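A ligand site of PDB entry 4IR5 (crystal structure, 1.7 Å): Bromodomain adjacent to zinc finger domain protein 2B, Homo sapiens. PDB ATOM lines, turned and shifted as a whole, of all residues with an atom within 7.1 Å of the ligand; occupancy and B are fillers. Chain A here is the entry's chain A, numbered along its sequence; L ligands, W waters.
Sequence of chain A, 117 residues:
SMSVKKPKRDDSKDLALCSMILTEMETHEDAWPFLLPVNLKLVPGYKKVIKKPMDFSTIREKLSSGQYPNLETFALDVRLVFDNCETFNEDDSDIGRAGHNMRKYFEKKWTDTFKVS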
ATOM      1  N   TRP A  32      -8.885   0.445 -26.290  1.00  0.00           N
ATOM      2  CA  TRP A  32      -9.647   0.017 -25.134  1.00  0.00           C
ATOM      3  C   TRP A  32     -10.349   1.114 -24.336  1.00  0.00           C
ATOM      4  O   TRP A  32     -11.428   0.822 -23.771  1.00  0.00           O
ATOM      5  CB  TRP A  32      -8.799  -0.859 -24.233  1.00  0.00           C
ATOM      6  CG  TRP A  32      -7.551  -0.202 -23.689  1.00  0.00           C
ATOM      7  CD1 TRP A  32      -6.275  -0.293 -24.247  1.00  0.00           C
ATOM      8  CD2 TRP A  32      -7.422   0.611 -22.536  1.00  0.00           C
ATOM      9  NE1 TRP A  32      -5.397   0.460 -23.510  1.00  0.00           N
ATOM     10  CE2 TRP A  32      -6.071   1.017 -22.443  1.00  0.00           C
ATOM     11  CE3 TRP A  32      -8.322   1.008 -21.524  1.00  0.00           C
ATOM     12  CZ2 TRP A  32      -5.616   1.819 -21.420  1.00  0.00           C
ATOM     13  CZ3 TRP A  32      -7.846   1.831 -20.524  1.00  0.00           C
ATOM     14  CH2 TRP A  32      -6.513   2.217 -20.466  1.00  0.00           C
ATOM     15  N   PRO A  33      -9.783   2.352 -24.214  1.00  0.00           N
ATOM     16  CA  PRO A  33     -10.542   3.368 -23.452  1.00  0.00           C
ATOM     17  C   PRO A  33     -11.812   3.856 -24.152  1.00  0.00           C
ATOM     18  O   PRO A  33     -12.619   4.506 -23.534  1.00  0.00           O
ATOM     19  CB  PRO A  33      -9.527   4.556 -23.289  1.00  0.00           C
ATOM     20  CG  PRO A  33      -8.186   3.956 -23.547  1.00  0.00           C
ATOM     21  CD  PRO A  33      -8.455   2.889 -24.600  1.00  0.00           C
ATOM     22  N   PHE A  34     -11.924   3.605 -25.457  1.00  0.00           N
ATOM     23  CA  PHE A  34     -12.840   4.294 -26.342  1.00  0.00           C
ATOM     24  C   PHE A  34     -13.943   3.396 -26.897  1.00  0.00           C
ATOM     25  O   PHE A  34     -14.737   3.831 -27.715  1.00  0.00           O
ATOM     26  CB  PHE A  34     -12.061   4.928 -27.505  1.00  0.00           C
ATOM     27  CG  PHE A  34     -10.881   5.724 -27.060  1.00  0.00           C
ATOM     28  CD1 PHE A  34     -11.053   6.838 -26.245  1.00  0.00           C
ATOM     29  CD2 PHE A  34      -9.592   5.320 -27.323  1.00  0.00           C
ATOM     30  CE1 PHE A  34      -9.975   7.543 -25.739  1.00  0.00           C
ATOM     31  CE2 PHE A  34      -8.483   6.021 -26.824  1.00  0.00           C
ATOM     32  CZ  PHE A  34      -8.676   7.134 -26.010  1.00  0.00           C
ATOM     33  N   LEU A  36     -16.557   1.800 -25.515  1.00  0.00           N
ATOM     34  CA  LEU A  36     -17.886   2.039 -24.945  1.00  0.00           C
ATOM     35  C   LEU A  36     -17.943   3.440 -24.368  1.00  0.00           C
ATOM     36  O   LEU A  36     -16.906   4.004 -24.001  1.00  0.00           O
ATOM     37  CB  LEU A  36     -18.185   1.025 -23.843  1.00  0.00           C
ATOM     38  CG  LEU A  36     -18.242  -0.432 -24.322  1.00  0.00           C
ATOM     39  CD1 LEU A  36     -18.372  -1.442 -23.191  1.00  0.00           C
ATOM     40  CD2 LEU A  36     -19.367  -0.650 -25.336  1.00  0.00           C
ATOM     41  N   PRO A  37     -19.163   3.965 -24.117  1.00  0.00           N
ATOM     42  CA  PRO A  37     -19.273   5.241 -23.420  1.00  0.00           C
ATOM     43  C   PRO A  37     -18.506   5.152 -22.087  1.00  0.00           C
ATOM     44  O   PRO A  37     -18.537   4.094 -21.402  1.00  0.00           O
ATOM     45  CB  PRO A  37     -20.777   5.377 -23.159  1.00  0.00           C
ATOM     46  CG  PRO A  37     -21.389   4.593 -24.272  1.00  0.00           C
ATOM     47  CD  PRO A  37     -20.479   3.423 -24.511  1.00  0.00           C
ATOM     48  N   VAL A  38     -17.888   6.247 -21.735  1.00  0.00           N
ATOM     49  CA  VAL A  38     -17.326   6.396 -20.380  1.00  0.00           C
ATOM     50  C   VAL A  38     -18.446   6.225 -19.364  1.00  0.00           C
ATOM     51  O   VAL A  38     -19.529   6.802 -19.546  1.00  0.00           O
ATOM     52  CB  VAL A  38     -16.636   7.771 -20.183  1.00  0.00           C
ATOM     53  CG1 VAL A  38     -16.188   7.947 -18.745  1.00  0.00           C
ATOM     54  CG2 VAL A  38     -15.477   7.928 -21.143  1.00  0.00           C
ATOM     55  N   ASN A  39     -18.254   5.380 -18.363  1.00  0.00           N
ATOM     56  CA  ASN A  39     -19.297   5.044 -17.464  1.00  0.00           C
ATOM     57  C   ASN A  39     -19.518   6.187 -16.447  1.00  0.00           C
ATOM     58  O   ASN A  39     -18.677   6.411 -15.581  1.00  0.00           O
ATOM     59  CB  ASN A  39     -18.975   3.730 -16.734  1.00  0.00           C
ATOM     60  CG  ASN A  39     -20.088   3.302 -15.796  1.00  0.00           C
ATOM     61  OD1 ASN A  39     -20.881   4.109 -15.342  1.00  0.00           O
ATOM     62  ND2 ASN A  39     -20.149   2.009 -15.519  1.00  0.00           N
ATOM     63  N   LEU A  40     -20.643   6.868 -16.613  1.00  0.00           N
ATOM     64  CA  LEU A  40     -20.901   8.168 -15.974  1.00  0.00           C
ATOM     65  C   LEU A  40     -21.219   8.030 -14.526  1.00  0.00           C
ATOM     66  O   LEU A  40     -21.216   9.045 -13.795  1.00  0.00           O
ATOM     67  CB  LEU A  40     -22.045   8.900 -16.675  1.00  0.00           C
ATOM     68  CG  LEU A  40     -21.873   9.357 -18.100  1.00  0.00           C
ATOM     69  CD1 LEU A  40     -23.089  10.157 -18.554  1.00  0.00           C
ATOM     70  CD2 LEU A  40     -20.600  10.166 -18.232  1.00  0.00           C
ATOM     71  N   LEU A  42     -19.485   5.756 -12.734  1.00  0.00           N
ATOM     72  CA  LEU A  42     -18.204   5.231 -12.268  1.00  0.00           C
ATOM     73  C   LEU A  42     -17.016   6.228 -12.342  1.00  0.00           C
ATOM     74  O   LEU A  42     -15.936   5.994 -11.747  1.00  0.00           O
ATOM     75  CB  LEU A  42     -17.870   3.985 -13.088  1.00  0.00           C
ATOM     76  CG  LEU A  42     -16.576   3.206 -12.831  1.00  0.00           C
ATOM     77  CD1 LEU A  42     -16.848   1.709 -12.933  1.00  0.00           C
ATOM     78  CD2 LEU A  42     -15.471   3.590 -13.802  1.00  0.00           C
ATOM     79  N   VAL A  43     -17.161   7.293 -13.134  1.00  0.00           N
ATOM     80  CA  VAL A  43     -16.077   8.241 -13.348  1.00  0.00           C
ATOM     81  C   VAL A  43     -16.590   9.612 -12.847  1.00  0.00           C
ATOM     82  O   VAL A  43     -17.311  10.292 -13.588  1.00  0.00           O
ATOM     83  CB  VAL A  43     -15.657   8.352 -14.821  1.00  0.00           C
ATOM     84  CG1 VAL A  43     -14.484   9.291 -14.990  1.00  0.00           C
ATOM     85  CG2 VAL A  43     -15.331   6.977 -15.388  1.00  0.00           C
ATOM     86  N   PRO A  44     -16.247   9.972 -11.608  1.00  0.00           N
ATOM     87  CA  PRO A  44     -16.653  11.249 -11.010  1.00  0.00           C
ATOM     88  C   PRO A  44     -16.263  12.396 -11.929  1.00  0.00           C
ATOM     89  O   PRO A  44     -15.244  12.338 -12.590  1.00  0.00           O
ATOM     90  CB  PRO A  44     -15.848  11.298  -9.699  1.00  0.00           C
ATOM     91  CG  PRO A  44     -15.629   9.881  -9.334  1.00  0.00           C
ATOM     92  CD  PRO A  44     -15.544   9.114 -10.620  1.00  0.00           C
ATOM     93  N   TYR A  46     -17.155  13.262 -14.898  1.00  0.00           N
ATOM     94  CA  TYR A  46     -17.163  13.153 -16.353  1.00  0.00           C
ATOM     95  C   TYR A  46     -18.369  13.831 -16.989  1.00  0.00           C
ATOM     96  O   TYR A  46     -18.280  14.583 -17.966  1.00  0.00           O
ATOM     97  CB  TYR A  46     -17.049  11.688 -16.841  1.00  0.00           C
ATOM     98  CG  TYR A  46     -16.549  11.634 -18.257  1.00  0.00           C
ATOM     99  CD1 TYR A  46     -17.414  11.554 -19.330  1.00  0.00           C
ATOM    100  CD2 TYR A  46     -15.198  11.689 -18.513  1.00  0.00           C
ATOM    101  CE1 TYR A  46     -16.958  11.534 -20.651  1.00  0.00           C
ATOM    102  CE2 TYR A  46     -14.712  11.653 -19.823  1.00  0.00           C
ATOM    103  CZ  TYR A  46     -15.598  11.577 -20.888  1.00  0.00           C
ATOM    104  OH  TYR A  46     -15.114  11.592 -22.171  1.00  0.00           O
ATOM    105  N   ILE A  50     -17.438  16.962 -19.432  1.00  0.00           N
ATOM    106  CA  ILE A  50     -17.432  16.594 -20.871  1.00  0.00           C
ATOM    107  C   ILE A  50     -18.864  16.740 -21.384  1.00  0.00           C
ATOM    108  O   ILE A  50     -19.733  15.894 -21.115  1.00  0.00           O
ATOM    109  CB  ILE A  50     -16.900  15.149 -21.069  1.00  0.00           C
ATOM    110  CG1 ILE A  50     -15.424  15.046 -20.638  1.00  0.00           C
ATOM    111  CG2 ILE A  50     -16.981  14.701 -22.545  1.00  0.00           C
ATOM    112  CD1 ILE A  50     -14.483  16.047 -21.289  1.00  0.00           C
ATOM    113  N   MET A  54     -18.502  10.969 -26.402  1.00  0.00           N
ATOM    114  CA  MET A  54     -18.539  10.171 -27.606  1.00  0.00           C
ATOM    115  C   MET A  54     -17.575   9.019 -27.468  1.00  0.00           C
ATOM    116  O   MET A  54     -16.564   9.124 -26.777  1.00  0.00           O
ATOM    117  CB  MET A  54     -18.240  11.042 -28.866  1.00  0.00           C
ATOM    118  CG  MET A  54     -18.403  10.387 -30.222  1.00  0.00           C
ATOM    119  SD  MET A  54     -20.023   9.655 -30.471  1.00  0.00           S
ATOM    120  CE  MET A  54     -21.130  11.006 -30.128  1.00  0.00           C
ATOM    121  N   VAL A  81     -14.068  12.217 -29.761  1.00  0.00           N
ATOM    122  CA  VAL A  81     -13.559  11.195 -28.835  1.00  0.00           C
ATOM    123  C   VAL A  81     -12.188  11.634 -28.282  1.00  0.00           C
ATOM    124  O   VAL A  81     -11.939  11.630 -27.049  1.00  0.00           O
ATOM    125  CB  VAL A  81     -13.398   9.783 -29.505  1.00  0.00           C
ATOM    126  CG1 VAL A  81     -12.833   8.767 -28.510  1.00  0.00           C
ATOM    127  CG2 VAL A  81     -14.751   9.298 -30.018  1.00  0.00           C
ATOM    128  N   ASN A  84     -12.238  14.956 -26.211  1.00  0.00           N
ATOM    129  CA  ASN A  84     -12.721  14.662 -24.829  1.00  0.00           C
ATOM    130  C   ASN A  84     -11.616  14.045 -23.978  1.00  0.00           C
ATOM    131  O   ASN A  84     -11.440  14.411 -22.810  1.00  0.00           O
ATOM    132  CB  ASN A  84     -13.927  13.766 -24.841  1.00  0.00           C
ATOM    133  CG  ASN A  84     -15.178  14.452 -25.367  1.00  0.00           C
ATOM    134  OD1 ASN A  84     -15.264  15.690 -25.466  1.00  0.00           O
ATOM    135  ND2 ASN A  84     -16.151  13.639 -25.721  1.00  0.00           N
ATOM    136  N   CYS A  85     -10.885  13.092 -24.557  1.00  0.00           N
ATOM    137  CA  CYS A  85      -9.861  12.384 -23.877  1.00  0.00           C
ATOM    138  C   CYS A  85      -8.766  13.301 -23.370  1.00  0.00           C
ATOM    139  O   CYS A  85      -8.353  13.230 -22.206  1.00  0.00           O
ATOM    140  CB  CYS A  85      -9.275  11.290 -24.788  1.00  0.00           C
ATOM    141  SG  CYS A  85      -8.058  10.232 -24.027  1.00  0.00           S
ATOM    142  N   GLU A  86      -8.345  14.242 -24.222  1.00  0.00           N
ATOM    143  CA  GLU A  86      -7.336  15.216 -23.835  1.00  0.00           C
ATOM    144  C   GLU A  86      -7.858  16.180 -22.749  1.00  0.00           C
ATOM    145  O   GLU A  86      -7.121  16.568 -21.846  1.00  0.00           O
ATOM    146  CB  GLU A  86      -6.910  16.053 -25.033  1.00  0.00           C
ATOM    147  CG  GLU A  86      -6.057  15.356 -26.019  1.00  0.00           C
ATOM    148  CD  GLU A  86      -5.238  16.354 -26.849  1.00  0.00           C
ATOM    149  OE1 GLU A  86      -5.124  16.055 -28.020  1.00  0.00           O
ATOM    150  OE2 GLU A  86      -4.685  17.363 -26.332  1.00  0.00           O
ATOM    151  N   PHE A  88     -10.009  15.509 -20.335  1.00  0.00           N
ATOM    152  CA  PHE A  88     -10.221  14.846 -19.057  1.00  0.00           C
ATOM    153  C   PHE A  88      -9.002  14.144 -18.499  1.00  0.00           C
ATOM    154  O   PHE A  88      -8.888  13.964 -17.307  1.00  0.00           O
ATOM    155  CB  PHE A  88     -11.392  13.853 -19.171  1.00  0.00           C
ATOM    156  CG  PHE A  88     -12.022  13.548 -17.848  1.00  0.00           C
ATOM    157  CD1 PHE A  88     -12.911  14.429 -17.293  1.00  0.00           C
ATOM    158  CD2 PHE A  88     -11.732  12.396 -17.160  1.00  0.00           C
ATOM    159  CE1 PHE A  88     -13.479  14.198 -16.059  1.00  0.00           C
ATOM    160  CE2 PHE A  88     -12.300  12.139 -15.911  1.00  0.00           C
ATOM    161  CZ  PHE A  88     -13.169  13.052 -15.361  1.00  0.00           C
ATOM    162  N   ASN A  89      -8.079  13.763 -19.367  1.00  0.00           N
ATOM    163  CA  ASN A  89      -6.980  12.885 -18.967  1.00  0.00           C
ATOM    164  C   ASN A  89      -5.602  13.526 -19.143  1.00  0.00           C
ATOM    165  O   ASN A  89      -5.373  14.284 -20.128  1.00  0.00           O
ATOM    166  CB  ASN A  89      -6.976  11.587 -19.761  1.00  0.00           C
ATOM    167  CG  ASN A  89      -8.272  10.800 -19.573  1.00  0.00           C
ATOM    168  OD1 ASN A  89      -8.495  10.159 -18.530  1.00  0.00           O
ATOM    169  ND2 ASN A  89      -9.136  10.915 -20.518  1.00  0.00           N
ATOM    170  N   ILE A  95      -4.547   6.293 -20.480  1.00  0.00           N
ATOM    171  CA  ILE A  95      -5.639   6.672 -21.338  1.00  0.00           C
ATOM    172  C   ILE A  95      -5.233   7.882 -22.191  1.00  0.00           C
ATOM    173  O   ILE A  95      -5.554   7.903 -23.378  1.00  0.00           O
ATOM    174  CB  ILE A  95      -6.890   6.993 -20.497  1.00  0.00           C
ATOM    175  CG1 ILE A  95      -7.415   5.645 -19.873  1.00  0.00           C
ATOM    176  CG2 ILE A  95      -7.948   7.648 -21.323  1.00  0.00           C
ATOM    177  CD1 ILE A  95      -8.531   5.859 -18.878  1.00  0.00           C
HETATM  178  C1  LIG L   1     -11.995   7.809 -22.506  1.00  0.00           C
HETATM  179  C2  LIG L   1     -11.811   8.124 -21.037  1.00  0.00           C
HETATM  180  O1  LIG L   1     -11.636   9.275 -20.637  1.00  0.00           O
HETATM  181  C3  LIG L   1     -11.923   7.045 -20.097  1.00  0.00           C
HETATM  182  C4  LIG L   1     -12.180   5.736 -20.372  1.00  0.00           C
HETATM  183  C5  LIG L   1     -12.230   5.023 -19.136  1.00  0.00           C
HETATM  184  C6  LIG L   1     -12.462   3.589 -19.017  1.00  0.00           C
HETATM  185  C7  LIG L   1     -11.542   2.727 -19.618  1.00  0.00           C
HETATM  186  C8  LIG L   1     -11.724   1.347 -19.506  1.00  0.00           C
HETATM  187  C9  LIG L   1     -12.796   0.828 -18.814  1.00  0.00           C
HETATM  188  C10 LIG L   1     -13.715   1.672 -18.225  1.00  0.00           C
HETATM  189  C11 LIG L   1     -13.564   3.063 -18.299  1.00  0.00           C
HETATM  190  C12 LIG L   1     -14.588   3.957 -17.629  1.00  0.00           C
HETATM  191  O2  LIG L   1     -15.883   3.779 -18.173  1.00  0.00           O
HETATM  192  C13 LIG L   1     -11.935   5.941 -18.155  1.00  0.00           C
HETATM  193  C14 LIG L   1     -11.812   5.832 -16.749  1.00  0.00           C
HETATM  194  C15 LIG L   1     -11.499   6.934 -16.042  1.00  0.00           C
HETATM  195  O3  LIG L   1     -11.365   6.921 -14.670  1.00  0.00           O
HETATM  196  C16 LIG L   1     -11.165   5.736 -13.978  1.00  0.00           C
HETATM  197  C17 LIG L   1     -12.224   5.158 -13.308  1.00  0.00           C
HETATM  198  C18 LIG L   1     -12.004   3.979 -12.607  1.00  0.00           C
HETATM  199  C19 LIG L   1     -10.746   3.407 -12.548  1.00  0.00           C
HETATM  200  C20 LIG L   1      -9.688   4.016 -13.189  1.00  0.00           C
HETATM  201  C21 LIG L   1      -9.886   5.177 -13.937  1.00  0.00           C
HETATM  202  C22 LIG L   1     -11.335   8.164 -16.615  1.00  0.00           C
HETATM  203  C23 LIG L   1     -11.471   8.295 -17.965  1.00  0.00           C
HETATM  204  N1  LIG L   1     -11.762   7.207 -18.725  1.00  0.00           N
HETATM  205  O   HOH W   1     -12.720  10.037 -24.979  1.00  0.00           O
HETATM  206  O   HOH W   2     -12.589  11.120 -22.528  1.00  0.00           O
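N of Asn 39 is in hydrogen-bond range of O2 of the ligand (2.9 Å).
O1 of the ligand is in hydrogen-bond range of ND2 of Asn 89.
The backbone NH of Leu 42 lies within hydrogen-bond range of the side-chain amide oxygen of Asn 39, 3.4 Å away.
ND2 of Asn 89 is in hydrogen-bond range of O of Cys 85 (3.0 Å).
The side-chain sulfur (SG) of Cys 85 lies within hydrogen-bond range of the backbone carbonyl oxygen (O) of Ile 95, 3.5 Å away.
CZ3 of Trp 32 touches C7 of the ligand, 3.9 Å away.
Pro 33 touches the ligand (O to C4, 3.4 Å).
CE1 of Phe 34 touches C1 of the ligand (3.8 Å).
Val 38 touches the ligand (CG2 to C2, 3.7 Å).
Leu 42 touches the ligand (CD2 to C17, 3.6 Å).
Val 43 touches the ligand (CG1 to C22, 3.7 Å).
Tyr 46 touches the ligand.
CD1 of Ile 95 touches C13 of the ligand (3.5 Å).
Hydrophobic or aromatic side chains that line the ligand: Trp 32, Phe 34, Val 38, Leu 42, Val 43, Tyr 46 and Ile 95.
The nearest printed residue that does not touch the ligand is Phe 88 (4.2 Å).
Water W2 lies within hydrogen-bond range of the side-chain hydroxyl of Tyr 46, an oxygen (O1) of the ligand, the backbone NH of Cys 85 and the backbone carbonyl oxygen of Asn 84.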
